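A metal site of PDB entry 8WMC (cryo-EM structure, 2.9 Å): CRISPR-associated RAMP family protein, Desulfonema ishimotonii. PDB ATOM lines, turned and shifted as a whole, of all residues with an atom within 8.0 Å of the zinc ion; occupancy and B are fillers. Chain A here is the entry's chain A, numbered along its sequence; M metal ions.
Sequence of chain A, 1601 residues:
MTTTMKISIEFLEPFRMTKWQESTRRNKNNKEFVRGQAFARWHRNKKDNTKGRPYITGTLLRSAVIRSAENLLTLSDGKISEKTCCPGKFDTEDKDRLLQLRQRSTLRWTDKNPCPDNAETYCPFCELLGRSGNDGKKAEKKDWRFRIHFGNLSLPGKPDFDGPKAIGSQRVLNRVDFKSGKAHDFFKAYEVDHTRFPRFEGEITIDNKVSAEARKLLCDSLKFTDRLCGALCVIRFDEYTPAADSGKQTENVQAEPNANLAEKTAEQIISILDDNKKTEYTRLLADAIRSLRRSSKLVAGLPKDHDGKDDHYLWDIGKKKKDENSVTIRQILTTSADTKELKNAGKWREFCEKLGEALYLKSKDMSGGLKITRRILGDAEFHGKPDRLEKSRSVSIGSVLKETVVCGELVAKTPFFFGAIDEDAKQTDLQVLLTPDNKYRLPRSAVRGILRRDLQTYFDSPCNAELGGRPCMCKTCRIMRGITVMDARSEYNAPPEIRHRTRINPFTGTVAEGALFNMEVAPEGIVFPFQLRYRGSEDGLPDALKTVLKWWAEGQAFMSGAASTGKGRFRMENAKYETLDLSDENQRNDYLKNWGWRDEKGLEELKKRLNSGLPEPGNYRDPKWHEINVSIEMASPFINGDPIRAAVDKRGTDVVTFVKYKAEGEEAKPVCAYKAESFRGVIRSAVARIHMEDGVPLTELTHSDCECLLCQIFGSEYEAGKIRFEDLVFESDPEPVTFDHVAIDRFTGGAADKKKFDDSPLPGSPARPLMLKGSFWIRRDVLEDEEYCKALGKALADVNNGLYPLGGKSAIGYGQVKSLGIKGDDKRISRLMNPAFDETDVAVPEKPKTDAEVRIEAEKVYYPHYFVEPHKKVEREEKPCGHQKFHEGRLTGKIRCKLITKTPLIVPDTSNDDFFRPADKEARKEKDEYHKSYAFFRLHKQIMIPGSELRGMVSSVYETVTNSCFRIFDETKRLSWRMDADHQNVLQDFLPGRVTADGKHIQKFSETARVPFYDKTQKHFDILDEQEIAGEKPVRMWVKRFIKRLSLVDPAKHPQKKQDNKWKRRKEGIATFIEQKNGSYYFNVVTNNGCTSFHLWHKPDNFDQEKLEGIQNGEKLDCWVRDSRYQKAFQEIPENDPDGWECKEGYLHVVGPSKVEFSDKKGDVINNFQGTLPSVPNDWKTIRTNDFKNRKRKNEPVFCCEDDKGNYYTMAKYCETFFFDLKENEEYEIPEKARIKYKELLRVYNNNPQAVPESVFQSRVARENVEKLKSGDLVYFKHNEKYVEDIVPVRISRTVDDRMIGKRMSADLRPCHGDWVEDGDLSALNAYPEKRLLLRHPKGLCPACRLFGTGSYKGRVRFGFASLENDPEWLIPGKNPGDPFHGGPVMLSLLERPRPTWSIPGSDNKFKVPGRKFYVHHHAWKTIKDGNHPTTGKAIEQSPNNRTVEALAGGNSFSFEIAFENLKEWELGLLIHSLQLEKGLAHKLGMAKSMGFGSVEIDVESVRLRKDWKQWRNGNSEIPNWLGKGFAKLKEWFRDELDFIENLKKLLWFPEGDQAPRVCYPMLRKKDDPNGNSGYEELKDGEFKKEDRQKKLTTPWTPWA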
ATOM      1  N   VAL A 874      14.731  -0.226   6.010  1.00  0.00           N
ATOM      2  CA  VAL A 874      13.716   0.461   5.222  1.00  0.00           C
ATOM      3  C   VAL A 874      14.194   0.477   3.776  1.00  0.00           C
ATOM      4  O   VAL A 874      15.316   0.889   3.489  1.00  0.00           O
ATOM      5  CB  VAL A 874      13.470   1.887   5.739  1.00  0.00           C
ATOM      6  CG1 VAL A 874      12.313   2.539   4.988  1.00  0.00           C
ATOM      7  CG2 VAL A 874      13.212   1.873   7.235  1.00  0.00           C
ATOM      8  N   ARG A 876      14.261   2.059   0.486  1.00  0.00           N
ATOM      9  CA  ARG A 876      14.054   3.353  -0.145  1.00  0.00           C
ATOM     10  C   ARG A 876      14.372   3.280  -1.640  1.00  0.00           C
ATOM     11  O   ARG A 876      15.012   2.349  -2.120  1.00  0.00           O
ATOM     12  CB  ARG A 876      14.917   4.421   0.521  1.00  0.00           C
ATOM     13  CG  ARG A 876      14.742   4.498   2.020  1.00  0.00           C
ATOM     14  CD  ARG A 876      14.797   5.929   2.510  1.00  0.00           C
ATOM     15  NE  ARG A 876      15.011   6.001   3.957  1.00  0.00           N
ATOM     16  CZ  ARG A 876      14.119   6.362   4.871  1.00  0.00           C
ATOM     17  NH1 ARG A 876      12.876   6.677   4.552  1.00  0.00           N
ATOM     18  NH2 ARG A 876      14.494   6.404   6.148  1.00  0.00           N
ATOM     19  N   GLU A 959       1.705   1.570   7.004  1.00  0.00           N
ATOM     20  CA  GLU A 959       3.068   1.889   7.416  1.00  0.00           C
ATOM     21  C   GLU A 959       3.633   0.823   8.338  1.00  0.00           C
ATOM     22  O   GLU A 959       4.793   0.439   8.204  1.00  0.00           O
ATOM     23  CB  GLU A 959       3.101   3.256   8.109  1.00  0.00           C
ATOM     24  CG  GLU A 959       2.875   4.431   7.180  1.00  0.00           C
ATOM     25  CD  GLU A 959       2.414   5.670   7.924  1.00  0.00           C
ATOM     26  OE1 GLU A 959       2.856   5.868   9.068  1.00  0.00           O
ATOM     27  OE2 GLU A 959       1.620   6.446   7.354  1.00  0.00           O
ATOM     28  N   SER A 964       7.675   1.068   7.158  1.00  0.00           N
ATOM     29  CA  SER A 964       8.077   2.336   6.569  1.00  0.00           C
ATOM     30  C   SER A 964       8.571   3.272   7.678  1.00  0.00           C
ATOM     31  O   SER A 964       8.668   2.899   8.848  1.00  0.00           O
ATOM     32  CB  SER A 964       6.922   2.943   5.794  1.00  0.00           C
ATOM     33  OG  SER A 964       6.475   2.068   4.773  1.00  0.00           O
ATOM     34  N   CYS A 965       8.892   4.501   7.304  1.00  0.00           N
ATOM     35  CA  CYS A 965       9.353   5.494   8.261  1.00  0.00           C
ATOM     36  C   CYS A 965       8.188   6.016   9.096  1.00  0.00           C
ATOM     37  O   CYS A 965       7.014   5.824   8.764  1.00  0.00           O
ATOM     38  CB  CYS A 965      10.041   6.653   7.542  1.00  0.00           C
ATOM     39  SG  CYS A 965       8.914   7.824   6.743  1.00  0.00           S
ATOM     40  N   PHE A 966       8.516   6.683  10.188  1.00  0.00           N
ATOM     41  CA  PHE A 966       7.523   7.379  11.002  1.00  0.00           C
ATOM     42  C   PHE A 966       7.046   8.592  10.202  1.00  0.00           C
ATOM     43  O   PHE A 966       7.732   9.612  10.142  1.00  0.00           O
ATOM     44  CB  PHE A 966       8.100   7.794  12.339  1.00  0.00           C
ATOM     45  CG  PHE A 966       8.076   6.713  13.379  1.00  0.00           C
ATOM     46  CD1 PHE A 966       8.502   5.422  13.081  1.00  0.00           C
ATOM     47  CD2 PHE A 966       7.631   6.974  14.665  1.00  0.00           C
ATOM     48  CE1 PHE A 966       8.480   4.432  14.034  1.00  0.00           C
ATOM     49  CE2 PHE A 966       7.609   5.979  15.626  1.00  0.00           C
ATOM     50  CZ  PHE A 966       8.033   4.711  15.306  1.00  0.00           C
ATOM     51  N   ARG A 967       5.876   8.460   9.575  1.00  0.00           N
ATOM     52  CA  ARG A 967       5.430   9.474   8.616  1.00  0.00           C
ATOM     53  C   ARG A 967       5.233  10.828   9.277  1.00  0.00           C
ATOM     54  O   ARG A 967       5.627  11.866   8.727  1.00  0.00           O
ATOM     55  CB  ARG A 967       4.143   8.997   7.944  1.00  0.00           C
ATOM     56  CG  ARG A 967       3.624   9.912   6.843  1.00  0.00           C
ATOM     57  CD  ARG A 967       2.406   9.303   6.172  1.00  0.00           C
ATOM     58  NE  ARG A 967       1.827  10.197   5.172  1.00  0.00           N
ATOM     59  CZ  ARG A 967       2.206  10.279   3.904  1.00  0.00           C
ATOM     60  NH1 ARG A 967       3.197   9.537   3.426  1.00  0.00           N
ATOM     61  NH2 ARG A 967       1.583  11.122   3.091  1.00  0.00           N
ATOM     62  N   ASP A1308      17.408   5.788  10.142  1.00  0.00           N
ATOM     63  CA  ASP A1308      16.658   5.245   9.006  1.00  0.00           C
ATOM     64  C   ASP A1308      15.160   5.393   9.193  1.00  0.00           C
ATOM     65  O   ASP A1308      14.428   5.541   8.211  1.00  0.00           O
ATOM     66  CB  ASP A1308      17.028   3.774   8.805  1.00  0.00           C
ATOM     67  CG  ASP A1308      18.463   3.589   8.362  1.00  0.00           C
ATOM     68  OD1 ASP A1308      18.969   4.426   7.587  1.00  0.00           O
ATOM     69  OD2 ASP A1308      19.087   2.589   8.780  1.00  0.00           O
ATOM     70  N   LEU A1309      14.674   5.339  10.439  1.00  0.00           N
ATOM     71  CA  LEU A1309      13.252   5.366  10.723  1.00  0.00           C
ATOM     72  C   LEU A1309      12.669   6.769  10.851  1.00  0.00           C
ATOM     73  O   LEU A1309      11.462   6.906  11.037  1.00  0.00           O
ATOM     74  CB  LEU A1309      12.968   4.587  12.004  1.00  0.00           C
ATOM     75  CG  LEU A1309      13.177   3.076  11.927  1.00  0.00           C
ATOM     76  CD1 LEU A1309      13.296   2.470  13.315  1.00  0.00           C
ATOM     77  CD2 LEU A1309      12.050   2.400  11.144  1.00  0.00           C
ATOM     78  N   ARG A1310      13.499   7.815  10.751  1.00  0.00           N
ATOM     79  CA  ARG A1310      12.979   9.163  10.795  1.00  0.00           C
ATOM     80  C   ARG A1310      12.238   9.491   9.501  1.00  0.00           C
ATOM     81  O   ARG A1310      12.402   8.786   8.499  1.00  0.00           O
ATOM     82  CB  ARG A1310      14.108  10.158  11.023  1.00  0.00           C
ATOM     83  CG  ARG A1310      14.491  10.354  12.480  1.00  0.00           C
ATOM     84  CD  ARG A1310      15.865  10.980  12.611  1.00  0.00           C
ATOM     85  NE  ARG A1310      15.938  12.283  11.956  1.00  0.00           N
ATOM     86  CZ  ARG A1310      17.055  12.964  11.751  1.00  0.00           C
ATOM     87  NH1 ARG A1310      18.237  12.504  12.141  1.00  0.00           N
ATOM     88  NH2 ARG A1310      16.990  14.156  11.149  1.00  0.00           N
ATOM     89  N   PRO A1311      11.408  10.539   9.487  1.00  0.00           N
ATOM     90  CA  PRO A1311      10.723  10.911   8.250  1.00  0.00           C
ATOM     91  C   PRO A1311      11.711  11.233   7.138  1.00  0.00           C
ATOM     92  O   PRO A1311      12.791  11.783   7.372  1.00  0.00           O
ATOM     93  CB  PRO A1311       9.914  12.153   8.640  1.00  0.00           C
ATOM     94  CG  PRO A1311       9.834  12.144  10.108  1.00  0.00           C
ATOM     95  CD  PRO A1311      10.977  11.347  10.639  1.00  0.00           C
ATOM     96  N   CYS A1312      11.338  10.917   5.901  1.00  0.00           N
ATOM     97  CA  CYS A1312      12.197  11.115   4.712  1.00  0.00           C
ATOM     98  C   CYS A1312      12.450  12.613   4.588  1.00  0.00           C
ATOM     99  O   CYS A1312      13.613  12.998   4.760  1.00  0.00           O
ATOM    100  CB  CYS A1312      11.536  10.572   3.443  1.00  0.00           C
ATOM    101  SG  CYS A1312      10.998   8.849   3.514  1.00  0.00           S
ATOM    102  N   HIS A1313      11.414  13.425   4.404  1.00  0.00           N
ATOM    103  CA  HIS A1313      11.489  14.899   4.254  1.00  0.00           C
ATOM    104  C   HIS A1313      11.129  15.494   5.611  1.00  0.00           C
ATOM    105  O   HIS A1313       9.981  15.913   5.752  1.00  0.00           O
ATOM    106  CB  HIS A1313      10.597  15.328   3.087  1.00  0.00           C
ATOM    107  CG  HIS A1313      11.050  14.868   1.744  1.00  0.00           C
ATOM    108  ND1 HIS A1313      11.452  13.567   1.497  1.00  0.00           N
ATOM    109  CD2 HIS A1313      11.164  15.511   0.569  1.00  0.00           C
ATOM    110  CE1 HIS A1313      11.800  13.450   0.238  1.00  0.00           C
ATOM    111  NE2 HIS A1313      11.624  14.627  -0.351  1.00  0.00           N
ATOM    112  N   HIS A1337      16.295  12.741   2.804  1.00  0.00           N
ATOM    113  CA  HIS A1337      17.133  11.585   3.100  1.00  0.00           C
ATOM    114  C   HIS A1337      18.102  11.350   1.937  1.00  0.00           C
ATOM    115  O   HIS A1337      17.774  11.638   0.786  1.00  0.00           O
ATOM    116  CB  HIS A1337      16.256  10.352   3.316  1.00  0.00           C
ATOM    117  CG  HIS A1337      16.950   9.258   4.069  1.00  0.00           C
ATOM    118  ND1 HIS A1337      17.399   8.104   3.448  1.00  0.00           N
ATOM    119  CD2 HIS A1337      17.266   9.133   5.371  1.00  0.00           C
ATOM    120  CE1 HIS A1337      17.966   7.326   4.351  1.00  0.00           C
ATOM    121  NE2 HIS A1337      17.906   7.925   5.524  1.00  0.00           N
ATOM    122  N   GLY A1340      16.276   8.242  -0.628  1.00  0.00           N
ATOM    123  CA  GLY A1340      15.025   8.367  -1.371  1.00  0.00           C
ATOM    124  C   GLY A1340      13.817   8.222  -0.453  1.00  0.00           C
ATOM    125  O   GLY A1340      13.832   8.681   0.695  1.00  0.00           O
ATOM    126  N   LEU A1341      12.772   7.586  -0.978  1.00  0.00           N
ATOM    127  CA  LEU A1341      11.464   7.501  -0.345  1.00  0.00           C
ATOM    128  C   LEU A1341      11.110   6.060  -0.002  1.00  0.00           C
ATOM    129  O   LEU A1341      11.313   5.154  -0.814  1.00  0.00           O
ATOM    130  CB  LEU A1341      10.373   8.081  -1.257  1.00  0.00           C
ATOM    131  CG  LEU A1341      10.399   9.594  -1.489  1.00  0.00           C
ATOM    132  CD1 LEU A1341       9.431   9.966  -2.608  1.00  0.00           C
ATOM    133  CD2 LEU A1341      10.066  10.354  -0.215  1.00  0.00           C
ATOM    134  N   CYS A1342      10.568   5.865   1.194  1.00  0.00           N
ATOM    135  CA  CYS A1342      10.136   4.563   1.674  1.00  0.00           C
ATOM    136  C   CYS A1342       8.809   4.178   1.004  1.00  0.00           C
ATOM    137  O   CYS A1342       8.178   5.007   0.352  1.00  0.00           O
ATOM    138  CB  CYS A1342      10.007   4.608   3.192  1.00  0.00           C
ATOM    139  SG  CYS A1342       8.702   5.695   3.775  1.00  0.00           S
ATOM    140  N   PRO A1343       8.384   2.913   1.122  1.00  0.00           N
ATOM    141  CA  PRO A1343       7.149   2.492   0.435  1.00  0.00           C
ATOM    142  C   PRO A1343       5.911   3.272   0.839  1.00  0.00           C
ATOM    143  O   PRO A1343       5.033   3.494  -0.006  1.00  0.00           O
ATOM    144  CB  PRO A1343       7.027   1.013   0.796  1.00  0.00           C
ATOM    145  CG  PRO A1343       8.389   0.587   1.173  1.00  0.00           C
ATOM    146  CD  PRO A1343       9.023   1.775   1.818  1.00  0.00           C
ATOM    147  N   ALA A1344       5.798   3.686   2.097  1.00  0.00           N
ATOM    148  CA  ALA A1344       4.626   4.439   2.522  1.00  0.00           C
ATOM    149  C   ALA A1344       4.597   5.821   1.883  1.00  0.00           C
ATOM    150  O   ALA A1344       3.564   6.244   1.353  1.00  0.00           O
ATOM    151  CB  ALA A1344       4.602   4.566   4.049  1.00  0.00           C
ATOM    152  N   CYS A1345       5.731   6.534   1.898  1.00  0.00           N
ATOM    153  CA  CYS A1345       5.796   7.849   1.282  1.00  0.00           C
ATOM    154  C   CYS A1345       5.638   7.788  -0.225  1.00  0.00           C
ATOM    155  O   CYS A1345       5.252   8.802  -0.834  1.00  0.00           O
ATOM    156  CB  CYS A1345       7.117   8.538   1.648  1.00  0.00           C
ATOM    157  SG  CYS A1345       7.252   9.056   3.379  1.00  0.00           S
ATOM    158  N   ARG A1346       5.939   6.653  -0.850  1.00  0.00           N
ATOM    159  CA  ARG A1346       5.766   6.534  -2.298  1.00  0.00           C
ATOM    160  C   ARG A1346       4.295   6.508  -2.684  1.00  0.00           C
ATOM    161  O   ARG A1346       3.908   7.094  -3.704  1.00  0.00           O
ATOM    162  CB  ARG A1346       6.462   5.263  -2.806  1.00  0.00           C
ATOM    163  CG  ARG A1346       7.775   5.523  -3.528  1.00  0.00           C
ATOM    164  CD  ARG A1346       8.383   4.224  -4.030  1.00  0.00           C
ATOM    165  NE  ARG A1346       9.148   3.544  -2.984  1.00  0.00           N
ATOM    166  CZ  ARG A1346       9.389   2.242  -2.931  1.00  0.00           C
ATOM    167  NH1 ARG A1346       8.943   1.404  -3.865  1.00  0.00           N
ATOM    168  NH2 ARG A1346      10.095   1.760  -1.919  1.00  0.00           N
ATOM    169  N   GLY A1349       2.278   9.832  -0.892  1.00  0.00           N
ATOM    170  CA  GLY A1349       2.816  11.121  -1.288  1.00  0.00           C
ATOM    171  C   GLY A1349       3.471  11.863  -0.142  1.00  0.00           C
ATOM    172  O   GLY A1349       3.478  11.438   1.012  1.00  0.00           O
ATOM    173  N   THR A1350       4.055  13.001  -0.491  1.00  0.00           N
ATOM    174  CA  THR A1350       4.704  13.878   0.478  1.00  0.00           C
ATOM    175  C   THR A1350       4.572  15.312  -0.001  1.00  0.00           C
ATOM    176  O   THR A1350       3.826  15.599  -0.945  1.00  0.00           O
ATOM    177  CB  THR A1350       6.167  13.454   0.700  1.00  0.00           C
ATOM    178  OG1 THR A1350       6.795  14.354   1.635  1.00  0.00           O
ATOM    179  CG2 THR A1350       6.954  13.435  -0.602  1.00  0.00           C
HETATM  180 ZN    ZN M   1       8.993   7.912   4.416  1.00  0.00          ZN
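The backbone NH (N) of His 1337 is in hydrogen-bond range of the backbone carbonyl oxygen (O) of Cys 1312, at 3.3 Å.
The side-chain sulfur (SG) of Cys 1312 sits close to the guanidinium group (NH1) of Arg 876, 3.1 Å away.
The zinc ion is bound by the side-chain sulfur of Cys 1342 (2.3 Å), the side-chain sulfur of Cys 1345 (2.3 Å), the side-chain sulfur of Cys 965 (2.3 Å) and the side-chain sulfur of Cys 1312 (2.4 Å).
The zinc ion has four donor atoms within binding distance.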
